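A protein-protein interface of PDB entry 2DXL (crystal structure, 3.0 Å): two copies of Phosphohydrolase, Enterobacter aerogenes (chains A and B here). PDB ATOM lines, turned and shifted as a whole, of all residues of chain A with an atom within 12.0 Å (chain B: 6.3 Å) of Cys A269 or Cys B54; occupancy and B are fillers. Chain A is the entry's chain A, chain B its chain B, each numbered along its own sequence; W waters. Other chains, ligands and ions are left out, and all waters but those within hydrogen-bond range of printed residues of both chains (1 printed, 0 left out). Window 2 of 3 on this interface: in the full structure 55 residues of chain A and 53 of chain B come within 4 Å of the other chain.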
ATOM      1  N   LEU A 262      15.380 -16.663 -18.761  1.00  0.00           N
ATOM      2  CA  LEU A 262      14.411 -15.601 -18.484  1.00  0.00           C
ATOM      3  C   LEU A 262      14.838 -14.759 -17.306  1.00  0.00           C
ATOM      4  O   LEU A 262      15.389 -15.277 -16.344  1.00  0.00           O
ATOM      5  CB  LEU A 262      13.036 -16.173 -18.207  1.00  0.00           C
ATOM      6  CG  LEU A 262      12.401 -16.967 -19.341  1.00  0.00           C
ATOM      7  CD1 LEU A 262      11.058 -17.487 -18.884  1.00  0.00           C
ATOM      8  CD2 LEU A 262      12.274 -16.132 -20.610  1.00  0.00           C
ATOM      9  N   TYR A 263      14.600 -13.457 -17.381  1.00  0.00           N
ATOM     10  CA  TYR A 263      14.944 -12.580 -16.281  1.00  0.00           C
ATOM     11  C   TYR A 263      13.908 -12.776 -15.185  1.00  0.00           C
ATOM     12  O   TYR A 263      12.703 -12.679 -15.432  1.00  0.00           O
ATOM     13  CB  TYR A 263      15.010 -11.114 -16.733  1.00  0.00           C
ATOM     14  CG  TYR A 263      15.114 -10.129 -15.588  1.00  0.00           C
ATOM     15  CD1 TYR A 263      16.344  -9.869 -14.967  1.00  0.00           C
ATOM     16  CD2 TYR A 263      13.977  -9.472 -15.111  1.00  0.00           C
ATOM     17  CE1 TYR A 263      16.435  -8.960 -13.906  1.00  0.00           C
ATOM     18  CE2 TYR A 263      14.048  -8.578 -14.043  1.00  0.00           C
ATOM     19  CZ  TYR A 263      15.272  -8.321 -13.443  1.00  0.00           C
ATOM     20  OH  TYR A 263      15.320  -7.433 -12.382  1.00  0.00           O
ATOM     21  N   ASP A 264      14.384 -13.076 -13.983  1.00  0.00           N
ATOM     22  CA  ASP A 264      13.533 -13.236 -12.817  1.00  0.00           C
ATOM     23  C   ASP A 264      14.009 -12.266 -11.748  1.00  0.00           C
ATOM     24  O   ASP A 264      15.161 -12.311 -11.321  1.00  0.00           O
ATOM     25  CB  ASP A 264      13.571 -14.688 -12.328  1.00  0.00           C
ATOM     26  CG  ASP A 264      12.737 -14.913 -11.075  1.00  0.00           C
ATOM     27  OD1 ASP A 264      13.185 -14.524  -9.976  1.00  0.00           O
ATOM     28  OD2 ASP A 264      11.638 -15.503 -11.175  1.00  0.00           O
ATOM     29  N   GLU A 265      13.126 -11.384 -11.314  1.00  0.00           N
ATOM     30  CA  GLU A 265      13.520 -10.328 -10.398  1.00  0.00           C
ATOM     31  C   GLU A 265      14.134 -10.814  -9.074  1.00  0.00           C
ATOM     32  O   GLU A 265      15.056 -10.189  -8.543  1.00  0.00           O
ATOM     33  CB  GLU A 265      12.335  -9.424 -10.136  1.00  0.00           C
ATOM     34  CG  GLU A 265      12.678  -8.205  -9.316  1.00  0.00           C
ATOM     35  CD  GLU A 265      11.430  -7.431  -8.952  1.00  0.00           C
ATOM     36  OE1 GLU A 265      10.659  -7.078  -9.884  1.00  0.00           O
ATOM     37  OE2 GLU A 265      11.215  -7.188  -7.736  1.00  0.00           O
ATOM     38  N   ASN A 266      13.615 -11.921  -8.553  1.00  0.00           N
ATOM     39  CA  ASN A 266      14.099 -12.509  -7.307  1.00  0.00           C
ATOM     40  C   ASN A 266      15.464 -13.204  -7.450  1.00  0.00           C
ATOM     41  O   ASN A 266      16.248 -13.262  -6.500  1.00  0.00           O
ATOM     42  CB  ASN A 266      13.046 -13.476  -6.735  1.00  0.00           C
ATOM     43  CG  ASN A 266      13.668 -14.585  -5.841  1.00  0.00           C
ATOM     44  OD1 ASN A 266      13.613 -15.784  -6.178  1.00  0.00           O
ATOM     45  ND2 ASN A 266      14.282 -14.176  -4.714  1.00  0.00           N
ATOM     46  N   ILE A 267      15.731 -13.753  -8.629  1.00  0.00           N
ATOM     47  CA  ILE A 267      17.029 -14.340  -8.928  1.00  0.00           C
ATOM     48  C   ILE A 267      18.038 -13.214  -9.121  1.00  0.00           C
ATOM     49  O   ILE A 267      19.220 -13.350  -8.762  1.00  0.00           O
ATOM     50  CB  ILE A 267      16.955 -15.240 -10.176  1.00  0.00           C
ATOM     51  CG1 ILE A 267      16.409 -16.610  -9.804  1.00  0.00           C
ATOM     52  CG2 ILE A 267      18.304 -15.417 -10.817  1.00  0.00           C
ATOM     53  CD1 ILE A 267      15.909 -17.439 -11.008  1.00  0.00           C
ATOM     54  N   SER A 268      17.553 -12.101  -9.668  1.00  0.00           N
ATOM     55  CA  SER A 268      18.395 -10.954  -9.974  1.00  0.00           C
ATOM     56  C   SER A 268      18.970 -10.278  -8.735  1.00  0.00           C
ATOM     57  O   SER A 268      20.127  -9.872  -8.752  1.00  0.00           O
ATOM     58  CB  SER A 268      17.630  -9.932 -10.798  1.00  0.00           C
ATOM     59  OG  SER A 268      18.432  -8.794 -11.025  1.00  0.00           O
ATOM     60  N   CYS A 269      18.149 -10.140  -7.690  1.00  0.00           N
ATOM     61  CA  CYS A 269      18.559  -9.536  -6.413  1.00  0.00           C
ATOM     62  C   CYS A 269      18.063 -10.344  -5.214  1.00  0.00           C
ATOM     63  O   CYS A 269      17.020 -10.033  -4.639  1.00  0.00           O
ATOM     64  CB  CYS A 269      18.043  -8.111  -6.297  1.00  0.00           C
ATOM     65  SG  CYS A 269      18.693  -7.004  -7.518  1.00  0.00           S
ATOM     66  N   PRO A 270      18.805 -11.394  -4.829  1.00  0.00           N
ATOM     67  CA  PRO A 270      18.332 -12.271  -3.766  1.00  0.00           C
ATOM     68  C   PRO A 270      18.395 -11.618  -2.386  1.00  0.00           C
ATOM     69  O   PRO A 270      19.203 -10.712  -2.161  1.00  0.00           O
ATOM     70  CB  PRO A 270      19.302 -13.454  -3.840  1.00  0.00           C
ATOM     71  CG  PRO A 270      20.006 -13.304  -5.165  1.00  0.00           C
ATOM     72  CD  PRO A 270      20.094 -11.847  -5.364  1.00  0.00           C
ATOM     73  N   THR A 271      17.531 -12.068  -1.479  1.00  0.00           N
ATOM     74  CA  THR A 271      17.617 -11.652  -0.077  1.00  0.00           C
ATOM     75  C   THR A 271      18.006 -12.838   0.807  1.00  0.00           C
ATOM     76  O   THR A 271      19.108 -13.386   0.678  1.00  0.00           O
ATOM     77  CB  THR A 271      16.308 -10.980   0.437  1.00  0.00           C
ATOM     78  OG1 THR A 271      15.176 -11.686  -0.077  1.00  0.00           O
ATOM     79  CG2 THR A 271      16.227  -9.497   0.000  1.00  0.00           C
ATOM     80  N   PHE B  11      27.402  -4.574 -12.089  1.00  0.00           N
ATOM     81  CA  PHE B  11      28.234  -5.149 -11.013  1.00  0.00           C
ATOM     82  C   PHE B  11      27.403  -5.775  -9.902  1.00  0.00           C
ATOM     83  O   PHE B  11      26.355  -5.240  -9.510  1.00  0.00           O
ATOM     84  CB  PHE B  11      29.162  -4.101 -10.396  1.00  0.00           C
ATOM     85  CG  PHE B  11      30.320  -3.719 -11.270  1.00  0.00           C
ATOM     86  CD1 PHE B  11      30.319  -2.516 -11.959  1.00  0.00           C
ATOM     87  CD2 PHE B  11      31.419  -4.558 -11.401  1.00  0.00           C
ATOM     88  CE1 PHE B  11      31.389  -2.161 -12.768  1.00  0.00           C
ATOM     89  CE2 PHE B  11      32.488  -4.205 -12.209  1.00  0.00           C
ATOM     90  CZ  PHE B  11      32.472  -3.007 -12.893  1.00  0.00           C
ATOM     91  N   ARG B  12      27.869  -6.914  -9.407  1.00  0.00           N
ATOM     92  CA  ARG B  12      27.282  -7.524  -8.214  1.00  0.00           C
ATOM     93  C   ARG B  12      28.237  -7.324  -7.038  1.00  0.00           C
ATOM     94  O   ARG B  12      29.334  -6.808  -7.221  1.00  0.00           O
ATOM     95  CB  ARG B  12      26.949  -9.002  -8.451  1.00  0.00           C
ATOM     96  CG  ARG B  12      25.806  -9.232  -9.445  1.00  0.00           C
ATOM     97  CD  ARG B  12      24.402  -9.217  -8.807  1.00  0.00           C
ATOM     98  NE  ARG B  12      24.400  -8.679  -7.450  1.00  0.00           N
ATOM     99  CZ  ARG B  12      24.184  -9.404  -6.358  1.00  0.00           C
ATOM    100  NH1 ARG B  12      23.916 -10.706  -6.467  1.00  0.00           N
ATOM    101  NH2 ARG B  12      24.223  -8.826  -5.160  1.00  0.00           N
ATOM    102  N   TYR B  19      22.560 -13.363 -11.289  1.00  0.00           N
ATOM    103  CA  TYR B  19      21.647 -14.497 -11.355  1.00  0.00           C
ATOM    104  C   TYR B  19      22.247 -15.764 -10.766  1.00  0.00           C
ATOM    105  O   TYR B  19      21.666 -16.843 -10.907  1.00  0.00           O
ATOM    106  CB  TYR B  19      21.182 -14.753 -12.798  1.00  0.00           C
ATOM    107  CG  TYR B  19      20.786 -13.493 -13.528  1.00  0.00           C
ATOM    108  CD1 TYR B  19      21.165 -13.279 -14.845  1.00  0.00           C
ATOM    109  CD2 TYR B  19      20.056 -12.498 -12.886  1.00  0.00           C
ATOM    110  CE1 TYR B  19      20.814 -12.132 -15.505  1.00  0.00           C
ATOM    111  CE2 TYR B  19      19.707 -11.341 -13.545  1.00  0.00           C
ATOM    112  CZ  TYR B  19      20.096 -11.162 -14.850  1.00  0.00           C
ATOM    113  OH  TYR B  19      19.746 -10.000 -15.489  1.00  0.00           O
ATOM    114  N   VAL B  52      25.625  -0.803 -11.389  1.00  0.00           N
ATOM    115  CA  VAL B  52      25.423  -1.951 -10.506  1.00  0.00           C
ATOM    116  C   VAL B  52      24.091  -2.634 -10.824  1.00  0.00           C
ATOM    117  O   VAL B  52      23.246  -2.071 -11.516  1.00  0.00           O
ATOM    118  CB  VAL B  52      25.475  -1.564  -9.016  1.00  0.00           C
ATOM    119  CG1 VAL B  52      26.858  -1.056  -8.645  1.00  0.00           C
ATOM    120  CG2 VAL B  52      24.428  -0.537  -8.701  1.00  0.00           C
ATOM    121  N   ASN B  53      23.890  -3.844 -10.321  1.00  0.00           N
ATOM    122  CA  ASN B  53      22.687  -4.580 -10.697  1.00  0.00           C
ATOM    123  C   ASN B  53      21.489  -4.368  -9.788  1.00  0.00           C
ATOM    124  O   ASN B  53      20.365  -4.385 -10.267  1.00  0.00           O
ATOM    125  CB  ASN B  53      22.965  -6.072 -10.859  1.00  0.00           C
ATOM    126  CG  ASN B  53      21.786  -6.813 -11.429  1.00  0.00           C
ATOM    127  OD1 ASN B  53      21.204  -7.668 -10.771  1.00  0.00           O
ATOM    128  ND2 ASN B  53      21.408  -6.471 -12.644  1.00  0.00           N
ATOM    129  N   CYS B  54      21.729  -4.179  -8.491  1.00  0.00           N
ATOM    130  CA  CYS B  54      20.655  -3.991  -7.521  1.00  0.00           C
ATOM    131  C   CYS B  54      20.654  -2.633  -6.828  1.00  0.00           C
ATOM    132  O   CYS B  54      19.721  -2.309  -6.117  1.00  0.00           O
ATOM    133  CB  CYS B  54      20.740  -5.048  -6.446  1.00  0.00           C
ATOM    134  SG  CYS B  54      20.649  -6.725  -7.024  1.00  0.00           S
ATOM    135  N   GLY B  55      21.698  -1.839  -7.005  1.00  0.00           N
ATOM    136  CA  GLY B  55      21.777  -0.552  -6.329  1.00  0.00           C
ATOM    137  C   GLY B  55      22.158  -0.680  -4.864  1.00  0.00           C
ATOM    138  O   GLY B  55      21.887   0.220  -4.072  1.00  0.00           O
ATOM    139  N   ARG B  56      22.787  -1.796  -4.501  1.00  0.00           N
ATOM    140  CA  ARG B  56      23.265  -2.018  -3.136  1.00  0.00           C
ATOM    141  C   ARG B  56      24.660  -1.409  -2.942  1.00  0.00           C
ATOM    142  O   ARG B  56      25.440  -1.358  -3.899  1.00  0.00           O
ATOM    143  CB  ARG B  56      23.260  -3.513  -2.833  1.00  0.00           C
ATOM    144  CG  ARG B  56      21.882  -4.124  -2.985  1.00  0.00           C
ATOM    145  CD  ARG B  56      21.899  -5.645  -2.930  1.00  0.00           C
ATOM    146  NE  ARG B  56      20.542  -6.203  -2.838  1.00  0.00           N
ATOM    147  CZ  ARG B  56      20.244  -7.484  -3.022  1.00  0.00           C
ATOM    148  NH1 ARG B  56      21.198  -8.342  -3.320  1.00  0.00           N
ATOM    149  NH2 ARG B  56      18.999  -7.907  -2.917  1.00  0.00           N
ATOM    150  N   GLU B  59      27.712  -3.390  -3.881  1.00  0.00           N
ATOM    151  CA  GLU B  59      27.880  -3.423  -5.322  1.00  0.00           C
ATOM    152  C   GLU B  59      28.661  -2.208  -5.820  1.00  0.00           C
ATOM    153  O   GLU B  59      29.529  -2.335  -6.684  1.00  0.00           O
ATOM    154  CB  GLU B  59      26.525  -3.490  -6.005  1.00  0.00           C
ATOM    155  CG  GLU B  59      25.826  -4.817  -5.873  1.00  0.00           C
ATOM    156  CD  GLU B  59      24.472  -4.800  -6.537  1.00  0.00           C
ATOM    157  OE1 GLU B  59      23.860  -3.714  -6.575  1.00  0.00           O
ATOM    158  OE2 GLU B  59      24.015  -5.858  -7.023  1.00  0.00           O
ATOM    159  N   HIS B  81      18.799   0.495 -12.868  1.00  0.00           N
ATOM    160  CA  HIS B  81      19.306  -0.434 -11.869  1.00  0.00           C
ATOM    161  C   HIS B  81      20.097   0.266 -10.784  1.00  0.00           C
ATOM    162  O   HIS B  81      20.316  -0.296  -9.699  1.00  0.00           O
ATOM    163  CB  HIS B  81      20.118  -1.554 -12.518  1.00  0.00           C
ATOM    164  CG  HIS B  81      19.265  -2.652 -13.077  1.00  0.00           C
ATOM    165  ND1 HIS B  81      18.567  -2.523 -14.262  1.00  0.00           N
ATOM    166  CD2 HIS B  81      18.969  -3.886 -12.600  1.00  0.00           C
ATOM    167  CE1 HIS B  81      17.885  -3.632 -14.493  1.00  0.00           C
ATOM    168  NE2 HIS B  81      18.113  -4.476 -13.500  1.00  0.00           N
ATOM    169  N   ASP B  82      20.478   1.507 -11.063  1.00  0.00           N
ATOM    170  CA  ASP B  82      21.268   2.295 -10.143  1.00  0.00           C
ATOM    171  C   ASP B  82      20.420   2.946  -9.051  1.00  0.00           C
ATOM    172  O   ASP B  82      19.187   3.002  -9.146  1.00  0.00           O
ATOM    173  CB  ASP B  82      22.066   3.327 -10.924  1.00  0.00           C
ATOM    174  CG  ASP B  82      23.285   2.719 -11.576  1.00  0.00           C
ATOM    175  OD1 ASP B  82      24.139   2.213 -10.816  1.00  0.00           O
ATOM    176  OD2 ASP B  82      23.389   2.716 -12.829  1.00  0.00           O
ATOM    177  N   ASP B  83      21.090   3.388  -7.991  1.00  0.00           N
ATOM    178  CA  ASP B  83      20.467   4.185  -6.944  1.00  0.00           C
ATOM    179  C   ASP B  83      21.173   5.535  -6.949  1.00  0.00           C
ATOM    180  O   ASP B  83      22.380   5.623  -6.697  1.00  0.00           O
ATOM    181  CB  ASP B  83      20.588   3.493  -5.583  1.00  0.00           C
ATOM    182  CG  ASP B  83      20.163   4.392  -4.432  1.00  0.00           C
ATOM    183  OD1 ASP B  83      18.956   4.455  -4.127  1.00  0.00           O
ATOM    184  OD2 ASP B  83      21.043   5.032  -3.820  1.00  0.00           O
HETATM  185  O   HOH W   1      22.327 -11.411  -9.175  1.00  0.00           O
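O of Cys A269 is in hydrogen-bond range of NH2 of Arg B56, at 3.4 Å.
SG of Cys A269 is disulfide-bonded to SG of Cys B54, at 2.0 Å.
The backbone carbonyl oxygen (O) of Ser A268 lies close to the side-chain sulfur (SG) of Cys B54 (3.6 Å).
OG of Ser A268 is in hydrogen-bond range of OD1 of Asn B53.
The guanidinium group (NH2) of Arg B56 lies within hydrogen-bond range of the backbone carbonyl oxygen (O) of Pro A270, 2.9 Å away.
The side-chain carboxylate of Glu B59 is in hydrogen-bond range of the backbone NH of Cys B54 (2.9 Å).
The side-chain carboxylate (OE1) of Glu B59 sits at hydrogen-bond distance from the backbone NH (N) of Arg B56 (3.0 Å).
The side-chain carboxylate (OD1) of Asp A264 sits at hydrogen-bond distance from the backbone NH (N) of Ile A267, at 3.0 Å.
The backbone carbonyl oxygen (O) of Phe B11 is in hydrogen-bond range of the backbone NH (N) of Asn B53 (2.9 Å).
Among the printed residues, merely in contact across the chains: Tyr A263 with Tyr B19 (3.4 Å), Ile A267 with Tyr B19 (3.5 Å) and Ser A268 with Tyr B19 (3.7 Å).
Of the printed residues of chain B, Tyr A263 touches Tyr B19.
Printed residues of chain A within 4 Å of Tyr B19: Tyr A263, Ile A267 and Ser A268.
No residue of chain A comes within 4 Å of Val B52.
Asn B53 touches just one residue of chain A: Ser A268.
No residue of chain A comes within 4 Å of Gly B55.
The nearest residue of chain B that does not touch Cys A269 is Asn B53 (4.1 Å).
The nearest residue of chain A that does not touch Cys B54 is Pro A270 (5.4 Å).
The nearest printed residue of chain B that does not touch Ser A268 is Arg B12 (4.3 Å).
Of the 10 printed residues of chain A, 5 touch a printed residue of chain B.
Hydrophobic or aromatic side chains of chain A that line the printed part of chain B: Tyr A263 and Ile A267.
Of the 12 printed residues of chain B, 4 touch a printed residue of chain A.
Hydrophobic or aromatic side chains of chain B within 4 Å of the printed part of chain A: Tyr B19.
No position is printed for both chains.
Of the 8 pairs that touch across the chains among the printed residues, none has its exchanged pair printed and touching as well.
Water W1 lies within hydrogen-bond range of O of Ser A268 (2.7 Å), N of Tyr B19 (2.9 Å) and NH1 of Arg B12 (3.2 Å).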
